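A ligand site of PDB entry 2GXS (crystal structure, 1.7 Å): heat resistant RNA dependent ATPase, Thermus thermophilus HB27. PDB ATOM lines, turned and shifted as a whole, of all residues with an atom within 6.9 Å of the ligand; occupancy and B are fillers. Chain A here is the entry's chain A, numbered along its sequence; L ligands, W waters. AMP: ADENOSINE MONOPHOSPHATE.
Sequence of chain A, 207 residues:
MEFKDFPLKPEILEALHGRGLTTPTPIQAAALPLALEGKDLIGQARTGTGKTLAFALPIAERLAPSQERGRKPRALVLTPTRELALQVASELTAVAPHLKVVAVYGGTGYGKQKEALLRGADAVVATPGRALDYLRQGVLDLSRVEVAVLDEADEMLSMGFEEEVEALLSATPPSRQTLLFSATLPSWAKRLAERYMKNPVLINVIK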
ATOM      1  N   PHE A   3      -1.581   8.599 -15.278  1.00  0.00           N
ATOM      2  CA  PHE A   3      -2.001   8.407 -16.673  1.00  0.00           C
ATOM      3  C   PHE A   3      -2.412   6.985 -16.927  1.00  0.00           C
ATOM      4  O   PHE A   3      -3.321   6.753 -17.668  1.00  0.00           O
ATOM      5  CB  PHE A   3      -0.897   8.793 -17.665  1.00  0.00           C
ATOM      6  CG  PHE A   3      -0.783  10.265 -17.875  1.00  0.00           C
ATOM      7  CD1 PHE A   3      -1.834  10.999 -18.480  1.00  0.00           C
ATOM      8  CD2 PHE A   3       0.335  10.963 -17.465  1.00  0.00           C
ATOM      9  CE1 PHE A   3      -1.735  12.355 -18.642  1.00  0.00           C
ATOM     10  CE2 PHE A   3       0.437  12.346 -17.639  1.00  0.00           C
ATOM     11  CZ  PHE A   3      -0.605  13.043 -18.220  1.00  0.00           C
ATOM     12  N   ARG A  19       8.703  10.286 -21.768  1.00  0.00           N
ATOM     13  CA  ARG A  19       8.956  11.702 -21.506  1.00  0.00           C
ATOM     14  C   ARG A  19       8.932  12.157 -20.054  1.00  0.00           C
ATOM     15  O   ARG A  19       9.094  13.353 -19.775  1.00  0.00           O
ATOM     16  CB  ARG A  19       7.969  12.546 -22.303  1.00  0.00           C
ATOM     17  CG  ARG A  19       8.090  12.347 -23.781  1.00  0.00           C
ATOM     18  CD  ARG A  19       6.820  12.800 -24.478  1.00  0.00           C
ATOM     19  NE  ARG A  19       6.559  14.204 -24.213  1.00  0.00           N
ATOM     20  CZ  ARG A  19       5.425  14.842 -24.510  1.00  0.00           C
ATOM     21  NH1 ARG A  19       4.401  14.191 -25.081  1.00  0.00           N
ATOM     22  NH2 ARG A  19       5.326  16.134 -24.228  1.00  0.00           N
ATOM     23  N   GLY A  20       8.784  11.223 -19.114  1.00  0.00           N
ATOM     24  CA  GLY A  20       8.824  11.554 -17.704  1.00  0.00           C
ATOM     25  C   GLY A  20       7.473  11.955 -17.161  1.00  0.00           C
ATOM     26  O   GLY A  20       7.365  12.493 -16.043  1.00  0.00           O
ATOM     27  N   LEU A  21       6.424  11.707 -17.957  1.00  0.00           N
ATOM     28  CA  LEU A  21       5.088  12.129 -17.617  1.00  0.00           C
ATOM     29  C   LEU A  21       4.288  10.958 -17.059  1.00  0.00           C
ATOM     30  O   LEU A  21       4.036   9.957 -17.804  1.00  0.00           O
ATOM     31  CB  LEU A  21       4.377  12.708 -18.845  1.00  0.00           C
ATOM     32  CG  LEU A  21       5.004  13.900 -19.543  1.00  0.00           C
ATOM     33  CD1 LEU A  21       4.260  14.210 -20.860  1.00  0.00           C
ATOM     34  CD2 LEU A  21       5.060  15.090 -18.624  1.00  0.00           C
ATOM     35  N   THR A  22       3.924  11.043 -15.771  1.00  0.00           N
ATOM     36  CA  THR A  22       3.158  10.020 -15.115  1.00  0.00           C
ATOM     37  C   THR A  22       1.871  10.479 -14.466  1.00  0.00           C
ATOM     38  O   THR A  22       0.964   9.674 -14.270  1.00  0.00           O
ATOM     39  CB  THR A  22       4.014   9.310 -13.989  1.00  0.00           C
ATOM     40  OG1 THR A  22       4.493  10.297 -13.068  1.00  0.00           O
ATOM     41  CG2 THR A  22       5.222   8.647 -14.584  1.00  0.00           C
ATOM     42  N   THR A  23       1.799  11.772 -14.160  1.00  0.00           N
ATOM     43  CA  THR A  23       0.733  12.280 -13.308  1.00  0.00           C
ATOM     44  C   THR A  23       0.013  13.417 -14.053  1.00  0.00           C
ATOM     45  O   THR A  23       0.638  14.440 -14.353  1.00  0.00           O
ATOM     46  CB  THR A  23       1.290  12.773 -11.989  1.00  0.00           C
ATOM     47  OG1 THR A  23       2.092  11.725 -11.406  1.00  0.00           O
ATOM     48  CG2 THR A  23       0.188  13.126 -11.051  1.00  0.00           C
ATOM     49  N   PRO A  24      -1.287  13.227 -14.341  1.00  0.00           N
ATOM     50  CA  PRO A  24      -1.980  14.332 -15.006  1.00  0.00           C
ATOM     51  C   PRO A  24      -2.013  15.610 -14.171  1.00  0.00           C
ATOM     52  O   PRO A  24      -2.141  15.554 -12.919  1.00  0.00           O
ATOM     53  CB  PRO A  24      -3.376  13.782 -15.244  1.00  0.00           C
ATOM     54  CG  PRO A  24      -3.514  12.547 -14.366  1.00  0.00           C
ATOM     55  CD  PRO A  24      -2.145  12.018 -14.271  1.00  0.00           C
ATOM     56  N   THR A  25      -1.950  16.765 -14.855  1.00  0.00           N
ATOM     57  CA  THR A  25      -2.181  18.059 -14.208  1.00  0.00           C
ATOM     58  C   THR A  25      -3.673  18.160 -13.874  1.00  0.00           C
ATOM     59  O   THR A  25      -4.488  17.323 -14.354  1.00  0.00           O
ATOM     60  CB  THR A  25      -1.792  19.232 -15.101  1.00  0.00           C
ATOM     61  OG1 THR A  25      -2.598  19.145 -16.283  1.00  0.00           O
ATOM     62  CG2 THR A  25      -0.321  19.130 -15.534  1.00  0.00           C
ATOM     63  N   ILE A  27      -6.102  20.159 -14.891  1.00  0.00           N
ATOM     64  CA  ILE A  27      -7.037  20.207 -16.037  1.00  0.00           C
ATOM     65  C   ILE A  27      -7.096  18.856 -16.773  1.00  0.00           C
ATOM     66  O   ILE A  27      -8.142  18.453 -17.249  1.00  0.00           O
ATOM     67  CB  ILE A  27      -6.724  21.345 -17.020  1.00  0.00           C
ATOM     68  CG1 ILE A  27      -7.959  21.574 -17.923  1.00  0.00           C
ATOM     69  CG2 ILE A  27      -5.442  21.095 -17.781  1.00  0.00           C
ATOM     70  CD1 ILE A  27      -8.018  22.980 -18.386  1.00  0.00           C
ATOM     71  N   GLN A  28      -5.969  18.147 -16.877  1.00  0.00           N
ATOM     72  CA  GLN A  28      -5.970  16.823 -17.512  1.00  0.00           C
ATOM     73  C   GLN A  28      -6.777  15.824 -16.705  1.00  0.00           C
ATOM     74  O   GLN A  28      -7.560  15.042 -17.254  1.00  0.00           O
ATOM     75  CB  GLN A  28      -4.543  16.330 -17.687  1.00  0.00           C
ATOM     76  CG  GLN A  28      -3.735  17.192 -18.602  1.00  0.00           C
ATOM     77  CD  GLN A  28      -2.209  17.002 -18.487  1.00  0.00           C
ATOM     78  OE1 GLN A  28      -1.721  16.279 -17.618  1.00  0.00           O
ATOM     79  NE2 GLN A  28      -1.456  17.698 -19.358  1.00  0.00           N
ATOM     80  N   ARG A  46      -4.628  28.516 -19.290  1.00  0.00           N
ATOM     81  CA  ARG A  46      -3.580  29.059 -20.183  1.00  0.00           C
ATOM     82  C   ARG A  46      -2.415  28.093 -20.287  1.00  0.00           C
ATOM     83  O   ARG A  46      -2.325  27.109 -19.507  1.00  0.00           O
ATOM     84  CB  ARG A  46      -3.017  30.345 -19.612  1.00  0.00           C
ATOM     85  CG  ARG A  46      -4.019  31.307 -19.084  1.00  0.00           C
ATOM     86  CD  ARG A  46      -3.325  32.544 -18.594  1.00  0.00           C
ATOM     87  NE  ARG A  46      -4.316  33.549 -18.261  1.00  0.00           N
ATOM     88  CZ  ARG A  46      -4.581  34.031 -17.062  1.00  0.00           C
ATOM     89  NH1 ARG A  46      -5.540  34.911 -16.945  1.00  0.00           N
ATOM     90  NH2 ARG A  46      -3.891  33.668 -15.976  1.00  0.00           N
ATOM     91  N   THR A  47      -1.467  28.363 -21.167  1.00  0.00           N
ATOM     92  CA  THR A  47      -0.221  27.602 -21.136  1.00  0.00           C
ATOM     93  C   THR A  47       0.365  27.690 -19.720  1.00  0.00           C
ATOM     94  O   THR A  47       0.254  28.755 -19.098  1.00  0.00           O
ATOM     95  CB  THR A  47       0.827  28.005 -22.191  1.00  0.00           C
ATOM     96  OG1 THR A  47       1.951  27.128 -22.032  1.00  0.00           O
ATOM     97  CG2 THR A  47       1.225  29.440 -22.083  1.00  0.00           C
ATOM     98  N   GLY A  48       0.919  26.550 -19.282  1.00  0.00           N
ATOM     99  CA  GLY A  48       1.428  26.243 -17.971  1.00  0.00           C
ATOM    100  C   GLY A  48       0.589  25.221 -17.219  1.00  0.00           C
ATOM    101  O   GLY A  48       1.067  24.582 -16.245  1.00  0.00           O
ATOM    102  N   THR A  49      -0.659  25.029 -17.701  1.00  0.00           N
ATOM    103  CA  THR A  49      -1.608  24.119 -17.040  1.00  0.00           C
ATOM    104  C   THR A  49      -1.586  22.661 -17.564  1.00  0.00           C
ATOM    105  O   THR A  49      -2.147  21.769 -16.937  1.00  0.00           O
ATOM    106  CB  THR A  49      -3.031  24.647 -17.250  1.00  0.00           C
ATOM    107  OG1 THR A  49      -3.287  24.735 -18.668  1.00  0.00           O
ATOM    108  CG2 THR A  49      -3.217  26.018 -16.649  1.00  0.00           C
ATOM    109  N   GLY A  50      -0.950  22.449 -18.723  1.00  0.00           N
ATOM    110  CA  GLY A  50      -1.040  21.173 -19.426  1.00  0.00           C
ATOM    111  C   GLY A  50      -2.276  20.997 -20.352  1.00  0.00           C
ATOM    112  O   GLY A  50      -2.659  19.867 -20.697  1.00  0.00           O
ATOM    113  N   LYS A  51      -2.877  22.097 -20.777  1.00  0.00           N
ATOM    114  CA  LYS A  51      -4.072  22.019 -21.607  1.00  0.00           C
ATOM    115  C   LYS A  51      -3.831  21.304 -22.941  1.00  0.00           C
ATOM    116  O   LYS A  51      -4.719  20.669 -23.487  1.00  0.00           O
ATOM    117  CB  LYS A  51      -4.683  23.417 -21.836  1.00  0.00           C
ATOM    118  CG  LYS A  51      -3.741  24.396 -22.548  1.00  0.00           C
ATOM    119  CD  LYS A  51      -4.378  25.744 -22.862  1.00  0.00           C
ATOM    120  CE  LYS A  51      -3.451  26.622 -23.633  1.00  0.00           C
ATOM    121  NZ  LYS A  51      -3.558  26.411 -25.085  1.00  0.00           N
ATOM    122  N   THR A  52      -2.606  21.380 -23.484  1.00  0.00           N
ATOM    123  CA  THR A  52      -2.382  20.757 -24.787  1.00  0.00           C
ATOM    124  C   THR A  52      -2.650  19.242 -24.762  1.00  0.00           C
ATOM    125  O   THR A  52      -3.369  18.725 -25.568  1.00  0.00           O
ATOM    126  CB  THR A  52      -0.955  21.054 -25.342  1.00  0.00           C
ATOM    127  OG1 THR A  52      -0.628  22.457 -25.240  1.00  0.00           O
ATOM    128  CG2 THR A  52      -0.892  20.623 -26.814  1.00  0.00           C
ATOM    129  N   LEU A  53      -2.088  18.514 -23.787  1.00  0.00           N
ATOM    130  CA  LEU A  53      -2.288  17.067 -23.721  1.00  0.00           C
ATOM    131  C   LEU A  53      -3.740  16.700 -23.355  1.00  0.00           C
ATOM    132  O   LEU A  53      -4.213  15.601 -23.662  1.00  0.00           O
ATOM    133  CB  LEU A  53      -1.294  16.484 -22.710  1.00  0.00           C
ATOM    134  CG  LEU A  53       0.109  16.194 -23.243  1.00  0.00           C
ATOM    135  CD1 LEU A  53       1.021  15.743 -22.061  1.00  0.00           C
ATOM    136  CD2 LEU A  53       0.068  15.140 -24.293  1.00  0.00           C
ATOM    137  N   ALA A  54      -4.440  17.618 -22.707  1.00  0.00           N
ATOM    138  CA  ALA A  54      -5.876  17.465 -22.370  1.00  0.00           C
ATOM    139  C   ALA A  54      -6.721  17.299 -23.633  1.00  0.00           C
ATOM    140  O   ALA A  54      -7.730  16.589 -23.586  1.00  0.00           O
ATOM    141  CB  ALA A  54      -6.371  18.658 -21.534  1.00  0.00           C
ATOM    142  N   PHE A  55      -6.330  17.927 -24.750  1.00  0.00           N
ATOM    143  CA  PHE A  55      -7.021  17.610 -26.039  1.00  0.00           C
ATOM    144  C   PHE A  55      -6.264  16.738 -27.016  1.00  0.00           C
ATOM    145  O   PHE A  55      -6.889  16.035 -27.832  1.00  0.00           O
ATOM    146  CB  PHE A  55      -7.506  18.874 -26.747  1.00  0.00           C
ATOM    147  CG  PHE A  55      -6.419  19.809 -27.222  1.00  0.00           C
ATOM    148  CD1 PHE A  55      -6.126  21.011 -26.562  1.00  0.00           C
ATOM    149  CD2 PHE A  55      -5.750  19.559 -28.416  1.00  0.00           C
ATOM    150  CE1 PHE A  55      -5.192  21.896 -27.075  1.00  0.00           C
ATOM    151  CE2 PHE A  55      -4.802  20.420 -28.915  1.00  0.00           C
ATOM    152  CZ  PHE A  55      -4.526  21.623 -28.269  1.00  0.00           C
ATOM    153  N   GLN A  87       3.628  24.345 -32.402  1.00  0.00           N
ATOM    154  CA  GLN A  87       3.734  23.690 -31.100  1.00  0.00           C
ATOM    155  C   GLN A  87       2.702  22.575 -30.949  1.00  0.00           C
ATOM    156  O   GLN A  87       3.034  21.465 -30.574  1.00  0.00           O
ATOM    157  CB  GLN A  87       3.558  24.675 -29.915  1.00  0.00           C
ATOM    158  CG  GLN A  87       4.750  25.636 -29.740  1.00  0.00           C
ATOM    159  CD  GLN A  87       4.467  26.863 -28.841  1.00  0.00           C
ATOM    160  OE1 GLN A  87       3.387  27.004 -28.254  1.00  0.00           O
ATOM    161  NE2 GLN A  87       5.465  27.737 -28.710  1.00  0.00           N
ATOM    162  N   GLU A  91       3.169  18.414 -30.587  1.00  0.00           N
ATOM    163  CA  GLU A  91       2.688  17.643 -29.471  1.00  0.00           C
ATOM    164  C   GLU A  91       1.688  16.586 -29.937  1.00  0.00           C
ATOM    165  O   GLU A  91       1.657  15.485 -29.376  1.00  0.00           O
ATOM    166  CB  GLU A  91       2.021  18.568 -28.474  1.00  0.00           C
ATOM    167  CG  GLU A  91       1.770  17.924 -27.126  1.00  0.00           C
ATOM    168  CD  GLU A  91       3.086  17.729 -26.329  1.00  0.00           C
ATOM    169  OE1 GLU A  91       4.183  18.163 -26.771  1.00  0.00           O
ATOM    170  OE2 GLU A  91       3.005  17.069 -25.297  1.00  0.00           O
ATOM    171  N   GLU A 152      -6.923  28.518 -27.279  1.00  0.00           N
ATOM    172  CA  GLU A 152      -6.692  29.927 -27.035  1.00  0.00           C
ATOM    173  C   GLU A 152      -7.702  30.803 -27.761  1.00  0.00           C
ATOM    174  O   GLU A 152      -7.359  31.732 -28.570  1.00  0.00           O
ATOM    175  CB  GLU A 152      -5.278  30.279 -27.339  1.00  0.00           C
ATOM    176  CG  GLU A 152      -4.359  29.447 -26.510  1.00  0.00           C
ATOM    177  CD  GLU A 152      -3.038  30.051 -26.314  1.00  0.00           C
ATOM    178  OE1 GLU A 152      -2.747  31.082 -26.976  1.00  0.00           O
ATOM    179  OE2 GLU A 152      -2.302  29.491 -25.492  1.00  0.00           O
HETATM  180  P   AMP L   1       0.715  23.547 -21.862  1.00  0.00           P
HETATM  181  O1P AMP L   1       1.387  24.582 -22.803  1.00  0.00           O
HETATM  182  O2P AMP L   1       0.017  22.510 -22.664  1.00  0.00           O
HETATM  183  O3P AMP L   1      -0.051  24.132 -20.672  1.00  0.00           O
HETATM  184  O5' AMP L   1       1.872  22.717 -21.077  1.00  0.00           O
HETATM  185  C5' AMP L   1       2.879  23.453 -20.394  1.00  0.00           C
HETATM  186  C4' AMP L   1       4.072  22.530 -20.077  1.00  0.00           C
HETATM  187  O4' AMP L   1       3.629  21.485 -19.200  1.00  0.00           O
HETATM  188  C3' AMP L   1       4.640  21.854 -21.327  1.00  0.00           C
HETATM  189  O3' AMP L   1       6.072  21.793 -21.304  1.00  0.00           O
HETATM  190  C2' AMP L   1       4.061  20.470 -21.198  1.00  0.00           C
HETATM  191  O2' AMP L   1       4.725  19.464 -21.939  1.00  0.00           O
HETATM  192  C1' AMP L   1       4.118  20.241 -19.731  1.00  0.00           C
HETATM  193  N9  AMP L   1       3.210  19.227 -19.226  1.00  0.00           N
HETATM  194  C8  AMP L   1       1.963  18.949 -19.701  1.00  0.00           C
HETATM  195  N7  AMP L   1       1.379  17.999 -18.983  1.00  0.00           N
HETATM  196  C5  AMP L   1       2.272  17.604 -18.022  1.00  0.00           C
HETATM  197  C6  AMP L   1       2.258  16.634 -16.948  1.00  0.00           C
HETATM  198  N6  AMP L   1       1.198  15.841 -16.766  1.00  0.00           N
HETATM  199  N1  AMP L   1       3.375  16.519 -16.158  1.00  0.00           N
HETATM  200  C2  AMP L   1       4.446  17.320 -16.344  1.00  0.00           C
HETATM  201  N3  AMP L   1       4.518  18.236 -17.322  1.00  0.00           N
HETATM  202  C4  AMP L   1       3.466  18.426 -18.181  1.00  0.00           C
HETATM  203  O   HOH W   1       6.889  19.988 -17.198  1.00  0.00           O
HETATM  204  O   HOH W   2       3.267  21.481 -15.985  1.00  0.00           O
HETATM  205  O   HOH W   3       7.257  18.577 -21.928  1.00  0.00           O
HETATM  206  O   HOH W   4       3.937  13.646 -14.622  1.00  0.00           O
HETATM  207  O   HOH W   5       7.505  21.825 -18.794  1.00  0.00           O
HETATM  208  O   HOH W   6       0.246  25.732 -24.824  1.00  0.00           O
HETATM  209  O   HOH W   7       3.209  23.958 -24.408  1.00  0.00           O
HETATM  210  O   HOH W   8       2.633  19.351 -23.808  1.00  0.00           O
HETATM  211  O   HOH W   9       0.284  19.704 -22.405  1.00  0.00           O
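Water W6 bridges O1P of the ligand (2.6 Å) and OG1 of Thr 52 (3.4 Å).
Water W8 lies within hydrogen-bond range of OE2 of Glu 91 (2.8 Å) and O2' of the ligand (2.8 Å).
Water W9 lies within hydrogen-bond range of an oxygen (O2P) of the ligand (2.8 Å), the backbone NH (N) of Leu 53 (3.0 Å) and the backbone carbonyl oxygen (O) of Gly 50 (3.4 Å).
Water W4 lies within hydrogen-bond range of N of Thr 22 (2.8 Å), N of Thr 23 (2.9 Å) and N1 of the ligand (3.3 Å).
N of Thr 52 is in hydrogen-bond range of O2P of the ligand, 3.0 Å away.
O2P of the ligand is in hydrogen-bond range of OG1 of Thr 52.
The side-chain hydroxyl (OG1) of Thr 47 sits at hydrogen-bond distance from an oxygen (O1P) of the ligand (2.7 Å).
O3P of the ligand is in hydrogen-bond range of N of Gly 50 (2.7 Å).
O of Thr 23 is in hydrogen-bond range of N6 of the ligand (2.8 Å).
NE2 of Gln 28 sits at hydrogen-bond distance from N7 of the ligand (2.9 Å).
The backbone NH (N) of Gly 48 lies within hydrogen-bond range of an oxygen (O3P) of the ligand, at 3.0 Å.
The backbone NH of Thr 49 lies within hydrogen-bond range of an oxygen (O3P) of the ligand, 3.2 Å away.
An oxygen (O2P) of the ligand sits at hydrogen-bond distance from the backbone NH (N) of Lys 51 (3.5 Å).
Merely in contact with the ligand: Phe 3 (3.6 Å), Leu 21 (3.2 Å), Pro 24 (3.9 Å), Thr 25 (3.8 Å), Arg 46 (3.9 Å) and Leu 53 (3.8 Å).
Hydrophobic or aromatic side chains that line the ligand: Phe 3, Leu 21 and Leu 53.
The nearest printed residue that does not touch the ligand is Arg 19 (4.1 Å).
O of Gly 50 sits at hydrogen-bond distance from NE2 of Gln 28 (2.8 Å).
OG1 of Thr 22 lies within hydrogen-bond range of OG1 of Thr 23, 3.3 Å away.
OE1 of Gln 28 sits at hydrogen-bond distance from N of Thr 25.
OG1 of Thr 49 lies within hydrogen-bond range of N of Lys 51 (3.4 Å).
The backbone carbonyl oxygen (O) of Thr 49 is in hydrogen-bond range of the side-chain hydroxyl (OG1) of Thr 25 (2.7 Å).
O of Arg 46 sits at hydrogen-bond distance from OG1 of Thr 49, 2.7 Å away.
NZ of Lys 51 lies within salt-bridge range of OE2 of Glu 152 (3.4 Å).
N of Phe 3 lies within hydrogen-bond range of O of Thr 22.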
